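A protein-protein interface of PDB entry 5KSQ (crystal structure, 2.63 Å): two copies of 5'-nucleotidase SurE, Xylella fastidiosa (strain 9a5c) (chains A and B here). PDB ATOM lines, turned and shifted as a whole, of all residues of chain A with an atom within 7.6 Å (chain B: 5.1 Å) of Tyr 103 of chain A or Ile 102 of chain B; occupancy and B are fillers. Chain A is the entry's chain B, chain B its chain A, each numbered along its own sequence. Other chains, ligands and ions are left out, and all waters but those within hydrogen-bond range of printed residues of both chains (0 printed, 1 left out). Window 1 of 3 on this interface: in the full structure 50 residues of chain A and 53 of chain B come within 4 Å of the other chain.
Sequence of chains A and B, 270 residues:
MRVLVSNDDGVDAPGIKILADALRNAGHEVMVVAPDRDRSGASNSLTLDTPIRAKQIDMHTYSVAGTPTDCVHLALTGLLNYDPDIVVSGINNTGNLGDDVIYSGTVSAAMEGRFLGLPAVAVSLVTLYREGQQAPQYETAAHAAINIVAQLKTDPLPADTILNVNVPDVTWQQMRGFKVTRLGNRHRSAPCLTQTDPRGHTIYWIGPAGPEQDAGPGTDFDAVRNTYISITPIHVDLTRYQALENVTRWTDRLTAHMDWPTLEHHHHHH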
ATOM      1  N   ASP A   8      20.852  -3.190  13.486  1.00  0.00           N
ATOM      2  CA  ASP A   8      21.149  -1.896  12.875  1.00  0.00           C
ATOM      3  C   ASP A   8      22.184  -1.995  11.749  1.00  0.00           C
ATOM      4  O   ASP A   8      22.584  -0.982  11.174  1.00  0.00           O
ATOM      5  CB  ASP A   8      21.606  -0.880  13.929  1.00  0.00           C
ATOM      6  CG  ASP A   8      23.072  -1.034  14.299  1.00  0.00           C
ATOM      7  OD1 ASP A   8      23.535  -2.184  14.462  1.00  0.00           O
ATOM      8  OD2 ASP A   8      23.763  -0.003  14.426  1.00  0.00           O
ATOM      9  N   SER A  40      24.139   2.945  10.902  1.00  0.00           N
ATOM     10  CA  SER A  40      25.151   3.524  11.775  1.00  0.00           C
ATOM     11  C   SER A  40      25.818   4.724  11.114  1.00  0.00           C
ATOM     12  O   SER A  40      26.479   4.590  10.086  1.00  0.00           O
ATOM     13  CB  SER A  40      26.209   2.478  12.151  1.00  0.00           C
ATOM     14  OG  SER A  40      25.662   1.456  12.961  1.00  0.00           O
ATOM     15  N   GLY A  41      25.637   5.897  11.711  1.00  0.00           N
ATOM     16  CA  GLY A  41      26.179   7.125  11.166  1.00  0.00           C
ATOM     17  C   GLY A  41      25.111   8.196  11.088  1.00  0.00           C
ATOM     18  O   GLY A  41      25.383   9.335  10.704  1.00  0.00           O
ATOM     19  N   ALA A  42      23.888   7.825  11.453  1.00  0.00           N
ATOM     20  CA  ALA A  42      22.771   8.764  11.460  1.00  0.00           C
ATOM     21  C   ALA A  42      22.081   8.788  12.821  1.00  0.00           C
ATOM     22  O   ALA A  42      22.452   8.044  13.731  1.00  0.00           O
ATOM     23  CB  ALA A  42      21.779   8.416  10.363  1.00  0.00           C
ATOM     24  N   ASN A  44      19.232   8.327  15.786  1.00  0.00           N
ATOM     25  CA  ASN A  44      18.473   7.158  16.217  1.00  0.00           C
ATOM     26  C   ASN A  44      17.014   7.466  16.553  1.00  0.00           C
ATOM     27  O   ASN A  44      16.225   6.553  16.802  1.00  0.00           O
ATOM     28  CB  ASN A  44      19.152   6.498  17.422  1.00  0.00           C
ATOM     29  CG  ASN A  44      20.477   5.849  17.067  1.00  0.00           C
ATOM     30  OD1 ASN A  44      20.695   5.433  15.929  1.00  0.00           O
ATOM     31  ND2 ASN A  44      21.368   5.752  18.047  1.00  0.00           N
ATOM     32  N   ASN A  96      30.155  -3.117  21.896  1.00  0.00           N
ATOM     33  CA  ASN A  96      29.648  -1.871  22.459  1.00  0.00           C
ATOM     34  C   ASN A  96      29.954  -1.800  23.953  1.00  0.00           C
ATOM     35  O   ASN A  96      29.197  -2.315  24.776  1.00  0.00           O
ATOM     36  CB  ASN A  96      28.141  -1.734  22.222  1.00  0.00           C
ATOM     37  CG  ASN A  96      27.787  -1.615  20.751  1.00  0.00           C
ATOM     38  OD1 ASN A  96      27.878  -0.537  20.163  1.00  0.00           O
ATOM     39  ND2 ASN A  96      27.374  -2.725  20.150  1.00  0.00           N
ATOM     40  N   ASP A  99      31.674   4.009  27.616  1.00  0.00           N
ATOM     41  CA  ASP A  99      30.876   5.205  27.370  1.00  0.00           C
ATOM     42  C   ASP A  99      30.562   5.400  25.888  1.00  0.00           C
ATOM     43  O   ASP A  99      30.545   6.525  25.389  1.00  0.00           O
ATOM     44  CB  ASP A  99      31.571   6.444  27.943  1.00  0.00           C
ATOM     45  CG  ASP A  99      33.023   6.546  27.521  1.00  0.00           C
ATOM     46  OD1 ASP A  99      33.625   5.501  27.193  1.00  0.00           O
ATOM     47  OD2 ASP A  99      33.565   7.670  27.526  1.00  0.00           O
ATOM     48  N   ASP A 100      30.311   4.295  25.194  1.00  0.00           N
ATOM     49  CA  ASP A 100      29.901   4.336  23.795  1.00  0.00           C
ATOM     50  C   ASP A 100      28.493   3.771  23.659  1.00  0.00           C
ATOM     51  O   ASP A 100      27.920   3.755  22.570  1.00  0.00           O
ATOM     52  CB  ASP A 100      30.869   3.532  22.927  1.00  0.00           C
ATOM     53  CG  ASP A 100      32.294   4.040  23.015  1.00  0.00           C
ATOM     54  OD1 ASP A 100      32.656   4.936  22.224  1.00  0.00           O
ATOM     55  OD2 ASP A 100      33.054   3.540  23.871  1.00  0.00           O
ATOM     56  N   VAL A 101      27.945   3.310  24.779  1.00  0.00           N
ATOM     57  CA  VAL A 101      26.644   2.648  24.799  1.00  0.00           C
ATOM     58  C   VAL A 101      25.488   3.613  24.534  1.00  0.00           C
ATOM     59  O   VAL A 101      24.540   3.275  23.824  1.00  0.00           O
ATOM     60  CB  VAL A 101      26.414   1.921  26.144  1.00  0.00           C
ATOM     61  CG1 VAL A 101      25.055   1.240  26.166  1.00  0.00           C
ATOM     62  CG2 VAL A 101      27.522   0.910  26.394  1.00  0.00           C
ATOM     63  N   ILE A 102      25.581   4.816  25.093  1.00  0.00           N
ATOM     64  CA  ILE A 102      24.491   5.791  25.026  1.00  0.00           C
ATOM     65  C   ILE A 102      24.083   6.168  23.593  1.00  0.00           C
ATOM     66  O   ILE A 102      22.923   6.489  23.337  1.00  0.00           O
ATOM     67  CB  ILE A 102      24.814   7.066  25.852  1.00  0.00           C
ATOM     68  CG1 ILE A 102      23.575   7.958  25.988  1.00  0.00           C
ATOM     69  CG2 ILE A 102      25.983   7.830  25.244  1.00  0.00           C
ATOM     70  CD1 ILE A 102      23.795   9.193  26.831  1.00  0.00           C
ATOM     71  N   TYR A 103      25.028   6.107  22.660  1.00  0.00           N
ATOM     72  CA  TYR A 103      24.740   6.462  21.273  1.00  0.00           C
ATOM     73  C   TYR A 103      24.840   5.258  20.337  1.00  0.00           C
ATOM     74  O   TYR A 103      25.170   5.403  19.159  1.00  0.00           O
ATOM     75  CB  TYR A 103      25.672   7.583  20.802  1.00  0.00           C
ATOM     76  CG  TYR A 103      25.540   8.864  21.601  1.00  0.00           C
ATOM     77  CD1 TYR A 103      24.305   9.282  22.081  1.00  0.00           C
ATOM     78  CD2 TYR A 103      26.651   9.650  21.883  1.00  0.00           C
ATOM     79  CE1 TYR A 103      24.178  10.450  22.813  1.00  0.00           C
ATOM     80  CE2 TYR A 103      26.534  10.819  22.615  1.00  0.00           C
ATOM     81  CZ  TYR A 103      25.296  11.213  23.078  1.00  0.00           C
ATOM     82  OH  TYR A 103      25.174  12.375  23.806  1.00  0.00           O
ATOM     83  N   SER A 104      24.544   4.073  20.864  1.00  0.00           N
ATOM     84  CA  SER A 104      24.603   2.844  20.076  1.00  0.00           C
ATOM     85  C   SER A 104      23.281   2.539  19.374  1.00  0.00           C
ATOM     86  O   SER A 104      22.205   2.727  19.942  1.00  0.00           O
ATOM     87  CB  SER A 104      25.006   1.659  20.954  1.00  0.00           C
ATOM     88  OG  SER A 104      24.856   0.435  20.255  1.00  0.00           O
ATOM     89  N   GLY A 105      23.376   2.055  18.139  1.00  0.00           N
ATOM     90  CA  GLY A 105      22.201   1.712  17.359  1.00  0.00           C
ATOM     91  C   GLY A 105      21.546   0.415  17.799  1.00  0.00           C
ATOM     92  O   GLY A 105      20.319   0.316  17.841  1.00  0.00           O
ATOM     93  N   THR A 106      22.368  -0.579  18.125  1.00  0.00           N
ATOM     94  CA  THR A 106      21.875  -1.878  18.574  1.00  0.00           C
ATOM     95  C   THR A 106      21.096  -1.747  19.883  1.00  0.00           C
ATOM     96  O   THR A 106      20.052  -2.378  20.062  1.00  0.00           O
ATOM     97  CB  THR A 106      23.033  -2.882  18.764  1.00  0.00           C
ATOM     98  OG1 THR A 106      23.777  -3.000  17.543  1.00  0.00           O
ATOM     99  CG2 THR A 106      22.502  -4.252  19.160  1.00  0.00           C
ATOM    100  N   VAL A 107      21.609  -0.916  20.786  1.00  0.00           N
ATOM    101  CA  VAL A 107      20.969  -0.670  22.075  1.00  0.00           C
ATOM    102  C   VAL A 107      19.645   0.081  21.917  1.00  0.00           C
ATOM    103  O   VAL A 107      18.690  -0.163  22.656  1.00  0.00           O
ATOM    104  CB  VAL A 107      21.907   0.128  23.012  1.00  0.00           C
ATOM    105  CG1 VAL A 107      21.240   0.396  24.355  1.00  0.00           C
ATOM    106  CG2 VAL A 107      23.219  -0.615  23.208  1.00  0.00           C
ATOM    107  N   SER A 108      19.591   0.987  20.945  1.00  0.00           N
ATOM    108  CA  SER A 108      18.405   1.814  20.726  1.00  0.00           C
ATOM    109  C   SER A 108      17.161   0.991  20.390  1.00  0.00           C
ATOM    110  O   SER A 108      16.045   1.360  20.759  1.00  0.00           O
ATOM    111  CB  SER A 108      18.663   2.852  19.628  1.00  0.00           C
ATOM    112  OG  SER A 108      18.898   2.230  18.378  1.00  0.00           O
ATOM    113  N   MET A 111      15.922  -0.528  23.577  1.00  0.00           N
ATOM    114  CA  MET A 111      15.377   0.517  24.433  1.00  0.00           C
ATOM    115  C   MET A 111      13.904   0.764  24.118  1.00  0.00           C
ATOM    116  O   MET A 111      13.090   0.964  25.020  1.00  0.00           O
ATOM    117  CB  MET A 111      16.171   1.813  24.262  1.00  0.00           C
ATOM    118  CG  MET A 111      15.823   2.896  25.268  1.00  0.00           C
ATOM    119  SD  MET A 111      16.435   2.521  26.921  1.00  0.00           S
ATOM    120  CE  MET A 111      18.201   2.506  26.625  1.00  0.00           C
ATOM    121  N   PHE A 115      10.051   0.268  26.462  1.00  0.00           N
ATOM    122  CA  PHE A 115       9.101   1.368  26.587  1.00  0.00           C
ATOM    123  C   PHE A 115       7.668   0.892  26.360  1.00  0.00           C
ATOM    124  O   PHE A 115       6.717   1.521  26.825  1.00  0.00           O
ATOM    125  CB  PHE A 115       9.439   2.486  25.598  1.00  0.00           C
ATOM    126  CG  PHE A 115      10.637   3.301  25.988  1.00  0.00           C
ATOM    127  CD1 PHE A 115      11.083   3.320  27.298  1.00  0.00           C
ATOM    128  CD2 PHE A 115      11.316   4.056  25.044  1.00  0.00           C
ATOM    129  CE1 PHE A 115      12.184   4.072  27.659  1.00  0.00           C
ATOM    130  CE2 PHE A 115      12.418   4.810  25.400  1.00  0.00           C
ATOM    131  CZ  PHE A 115      12.853   4.817  26.709  1.00  0.00           C
ATOM    132  N   HIS A 187      37.319   8.006  27.126  1.00  0.00           N
ATOM    133  CA  HIS A 187      37.402   9.262  26.381  1.00  0.00           C
ATOM    134  C   HIS A 187      38.365  10.280  26.993  1.00  0.00           C
ATOM    135  O   HIS A 187      38.867  11.163  26.295  1.00  0.00           O
ATOM    136  CB  HIS A 187      36.013   9.887  26.223  1.00  0.00           C
ATOM    137  CG  HIS A 187      35.111   9.133  25.298  1.00  0.00           C
ATOM    138  ND1 HIS A 187      33.816   9.528  25.031  1.00  0.00           N
ATOM    139  CD2 HIS A 187      35.315   8.005  24.575  1.00  0.00           C
ATOM    140  CE1 HIS A 187      33.264   8.679  24.185  1.00  0.00           C
ATOM    141  NE2 HIS A 187      34.152   7.745  23.892  1.00  0.00           N
ATOM    142  N   HIS A 235      20.325   1.709  32.902  1.00  0.00           N
ATOM    143  CA  HIS A 235      19.102   2.458  33.182  1.00  0.00           C
ATOM    144  C   HIS A 235      18.169   2.558  31.980  1.00  0.00           C
ATOM    145  O   HIS A 235      18.577   2.341  30.838  1.00  0.00           O
ATOM    146  CB  HIS A 235      19.437   3.870  33.674  1.00  0.00           C
ATOM    147  CG  HIS A 235      19.977   3.916  35.070  1.00  0.00           C
ATOM    148  ND1 HIS A 235      19.175   3.778  36.182  1.00  0.00           N
ATOM    149  CD2 HIS A 235      21.236   4.100  35.534  1.00  0.00           C
ATOM    150  CE1 HIS A 235      19.918   3.867  37.271  1.00  0.00           C
ATOM    151  NE2 HIS A 235      21.171   4.062  36.906  1.00  0.00           N
ATOM    152  N   VAL A 236      16.914   2.898  32.252  1.00  0.00           N
ATOM    153  CA  VAL A 236      15.927   3.121  31.204  1.00  0.00           C
ATOM    154  C   VAL A 236      15.314   4.514  31.375  1.00  0.00           C
ATOM    155  O   VAL A 236      14.765   5.089  30.434  1.00  0.00           O
ATOM    156  CB  VAL A 236      14.833   2.025  31.219  1.00  0.00           C
ATOM    157  CG1 VAL A 236      13.971   2.135  32.469  1.00  0.00           C
ATOM    158  CG2 VAL A 236      13.980   2.092  29.961  1.00  0.00           C
ATOM    159  N   LEU A 238      16.367   8.378  32.621  1.00  0.00           N
ATOM    160  CA  LEU A 238      17.543   9.214  32.850  1.00  0.00           C
ATOM    161  C   LEU A 238      17.388  10.195  34.013  1.00  0.00           C
ATOM    162  O   LEU A 238      18.281  10.999  34.272  1.00  0.00           O
ATOM    163  CB  LEU A 238      17.927   9.973  31.577  1.00  0.00           C
ATOM    164  CG  LEU A 238      18.337   9.124  30.371  1.00  0.00           C
ATOM    165  CD1 LEU A 238      18.907   9.997  29.263  1.00  0.00           C
ATOM    166  CD2 LEU A 238      19.330   8.050  30.781  1.00  0.00           C
ATOM    167  N   ASN B  44      25.733  11.397  16.913  1.00  0.00           N
ATOM    168  CA  ASN B  44      26.441  12.257  17.857  1.00  0.00           C
ATOM    169  C   ASN B  44      27.754  11.663  18.369  1.00  0.00           C
ATOM    170  O   ASN B  44      28.441  12.275  19.186  1.00  0.00           O
ATOM    171  CB  ASN B  44      25.534  12.613  19.038  1.00  0.00           C
ATOM    172  CG  ASN B  44      24.332  13.439  18.621  1.00  0.00           C
ATOM    173  OD1 ASN B  44      24.387  14.190  17.647  1.00  0.00           O
ATOM    174  ND2 ASN B  44      23.239  13.306  19.364  1.00  0.00           N
ATOM    175  N   SER B  45      28.095  10.473  17.884  1.00  0.00           N
ATOM    176  CA  SER B  45      29.313   9.792  18.313  1.00  0.00           C
ATOM    177  C   SER B  45      30.574  10.478  17.782  1.00  0.00           C
ATOM    178  O   SER B  45      30.523  11.223  16.802  1.00  0.00           O
ATOM    179  CB  SER B  45      29.285   8.324  17.876  1.00  0.00           C
ATOM    180  N   THR B  69      30.174  17.037  19.821  1.00  0.00           N
ATOM    181  CA  THR B  69      31.048  16.333  20.754  1.00  0.00           C
ATOM    182  C   THR B  69      32.513  16.489  20.349  1.00  0.00           C
ATOM    183  O   THR B  69      33.403  16.482  21.199  1.00  0.00           O
ATOM    184  CB  THR B  69      30.694  14.834  20.871  1.00  0.00           C
ATOM    185  OG1 THR B  69      30.756  14.220  19.578  1.00  0.00           O
ATOM    186  CG2 THR B  69      29.298  14.657  21.450  1.00  0.00           C
ATOM    187  N   ASP B  99      11.304  11.835  26.342  1.00  0.00           N
ATOM    188  CA  ASP B  99      12.273  10.859  25.853  1.00  0.00           C
ATOM    189  C   ASP B  99      12.960  11.331  24.575  1.00  0.00           C
ATOM    190  O   ASP B  99      13.379  10.522  23.747  1.00  0.00           O
ATOM    191  CB  ASP B  99      11.619   9.489  25.644  1.00  0.00           C
ATOM    192  CG  ASP B  99      10.290   9.576  24.918  1.00  0.00           C
ATOM    193  OD1 ASP B  99      10.090  10.534  24.141  1.00  0.00           O
ATOM    194  OD2 ASP B  99       9.439   8.684  25.126  1.00  0.00           O
ATOM    195  N   ASP B 100      13.073  12.647  24.424  1.00  0.00           N
ATOM    196  CA  ASP B 100      13.765  13.236  23.284  1.00  0.00           C
ATOM    197  C   ASP B 100      15.134  13.734  23.731  1.00  0.00           C
ATOM    198  O   ASP B 100      15.962  14.139  22.915  1.00  0.00           O
ATOM    199  CB  ASP B 100      12.954  14.397  22.704  1.00  0.00           C
ATOM    200  CG  ASP B 100      11.566  13.977  22.266  1.00  0.00           C
ATOM    201  OD1 ASP B 100      11.011  13.030  22.862  1.00  0.00           O
ATOM    202  OD2 ASP B 100      11.026  14.597  21.325  1.00  0.00           O
ATOM    203  N   VAL B 101      15.360  13.696  25.040  1.00  0.00           N
ATOM    204  CA  VAL B 101      16.589  14.206  25.633  1.00  0.00           C
ATOM    205  C   VAL B 101      17.793  13.310  25.339  1.00  0.00           C
ATOM    206  O   VAL B 101      18.890  13.803  25.067  1.00  0.00           O
ATOM    207  CB  VAL B 101      16.431  14.378  27.161  1.00  0.00           C
ATOM    208  CG1 VAL B 101      17.708  14.926  27.778  1.00  0.00           C
ATOM    209  CG2 VAL B 101      15.253  15.291  27.470  1.00  0.00           C
ATOM    210  N   ILE B 102      17.580  11.997  25.380  1.00  0.00           N
ATOM    211  CA  ILE B 102      18.668  11.031  25.230  1.00  0.00           C
ATOM    212  C   ILE B 102      19.385  11.127  23.878  1.00  0.00           C
ATOM    213  O   ILE B 102      20.570  10.811  23.772  1.00  0.00           O
ATOM    214  CB  ILE B 102      18.179   9.580  25.492  1.00  0.00           C
ATOM    215  CG1 ILE B 102      19.364   8.610  25.571  1.00  0.00           C
ATOM    216  CG2 ILE B 102      17.172   9.143  24.434  1.00  0.00           C
ATOM    217  CD1 ILE B 102      18.969   7.171  25.823  1.00  0.00           C
ATOM    218  N   TYR B 103      18.673  11.585  22.852  1.00  0.00           N
ATOM    219  CA  TYR B 103      19.245  11.684  21.511  1.00  0.00           C
ATOM    220  C   TYR B 103      19.408  13.134  21.055  1.00  0.00           C
ATOM    221  O   TYR B 103      19.578  13.405  19.864  1.00  0.00           O
ATOM    222  CB  TYR B 103      18.385  10.908  20.510  1.00  0.00           C
ATOM    223  CG  TYR B 103      18.304   9.427  20.805  1.00  0.00           C
ATOM    224  CD1 TYR B 103      19.379   8.753  21.370  1.00  0.00           C
ATOM    225  CD2 TYR B 103      17.150   8.704  20.527  1.00  0.00           C
ATOM    226  CE1 TYR B 103      19.311   7.400  21.645  1.00  0.00           C
ATOM    227  CE2 TYR B 103      17.072   7.351  20.800  1.00  0.00           C
ATOM    228  CZ  TYR B 103      18.155   6.704  21.358  1.00  0.00           C
ATOM    229  OH  TYR B 103      18.085   5.357  21.631  1.00  0.00           O
ATOM    230  N   SER B 104      19.362  14.061  22.005  1.00  0.00           N
ATOM    231  CA  SER B 104      19.475  15.482  21.694  1.00  0.00           C
ATOM    232  C   SER B 104      20.910  15.887  21.374  1.00  0.00           C
ATOM    233  O   SER B 104      21.850  15.476  22.057  1.00  0.00           O
ATOM    234  CB  SER B 104      18.938  16.329  22.850  1.00  0.00           C
ATOM    235  OG  SER B 104      19.118  17.711  22.598  1.00  0.00           O
ATOM    236  N   VAL B 107      22.257  18.408  24.172  1.00  0.00           N
ATOM    237  CA  VAL B 107      22.644  17.715  25.398  1.00  0.00           C
ATOM    238  C   VAL B 107      23.983  16.988  25.242  1.00  0.00           C
ATOM    239  O   VAL B 107      24.768  16.903  26.190  1.00  0.00           O
ATOM    240  CB  VAL B 107      21.546  16.718  25.845  1.00  0.00           C
ATOM    241  CG1 VAL B 107      21.971  15.953  27.090  1.00  0.00           C
ATOM    242  CG2 VAL B 107      20.238  17.451  26.094  1.00  0.00           C
ATOM    243  N   SER B 108      24.246  16.484  24.039  1.00  0.00           N
ATOM    244  CA  SER B 108      25.457  15.711  23.764  1.00  0.00           C
ATOM    245  C   SER B 108      26.742  16.488  24.057  1.00  0.00           C
ATOM    246  O   SER B 108      27.742  15.909  24.485  1.00  0.00           O
ATOM    247  CB  SER B 108      25.461  15.209  22.317  1.00  0.00           C
ATOM    248  OG  SER B 108      25.442  16.287  21.399  1.00  0.00           O
ATOM    249  N   MET B 111      27.180  16.608  27.783  1.00  0.00           N
ATOM    250  CA  MET B 111      27.492  15.262  28.248  1.00  0.00           C
ATOM    251  C   MET B 111      28.992  14.977  28.155  1.00  0.00           C
ATOM    252  O   MET B 111      29.567  14.348  29.044  1.00  0.00           O
ATOM    253  CB  MET B 111      26.700  14.230  27.437  1.00  0.00           C
ATOM    254  CG  MET B 111      26.751  12.808  27.980  1.00  0.00           C
ATOM    255  SD  MET B 111      25.763  12.567  29.473  1.00  0.00           S
ATOM    256  CE  MET B 111      24.149  13.097  28.910  1.00  0.00           C
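Tyr 103 of chain A touches Ile 102 of chain B, but with the chains exchanged Ile 102 of chain A does not touch Tyr 103 of chain B (4.1 Å).
Tyr 103 of chain A touches Ser 108 of chain B, and with the chains exchanged Ser 108 of chain A touches Tyr 103 of chain B.
Positions printed for both chains: 44, 99, 100, 101, 102, 103, 104, 107, 108 and 111.
O of Ile 102 of chain B touches CE1 of Tyr 103 of chain A, 3.8 Å away.
Ser 108 of chain B touches Tyr 103 of chain A.
OH of Tyr 103 of chain B touches CB of Ser 108 of chain A, 3.3 Å away.
Leu 238 of chain A touches Ile 102 of chain B (CD1 to CB, 3.9 Å).
Ile 102 of chain B touches just these residues of chain A: Tyr 103 and Leu 238.
Printed residues of chain B within 4 Å of Leu 238 of chain A: Ile 102.
Of the printed residues of chain A, Tyr 103 of chain B touches Ser 108 (3.3 Å).
Ser 40 of chain A touches none of the printed residues of chain B.
Thr 106 of chain A touches none of the printed residues of chain B.
The nearest residue of chain B that does not touch Tyr 103 of chain A is Asn 44 of chain B (4.1 Å).
Printed residues of chain A that touch a printed residue of chain B: Tyr 103, Ser 108 and Leu 238.
Hydrophobic or aromatic side chains of chain A that line the printed part of chain B: Tyr 103 and Leu 238.
Of the 12 printed residues of chain B, 3 touch a printed residue of chain A.
Printed residues of chain B that touch a printed residue of chain A: Ile 102, Tyr 103 and Ser 108.
OG of Ser 108 of chain A sits at hydrogen-bond distance from O of Gly 105 of chain A, at 2.4 Å.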
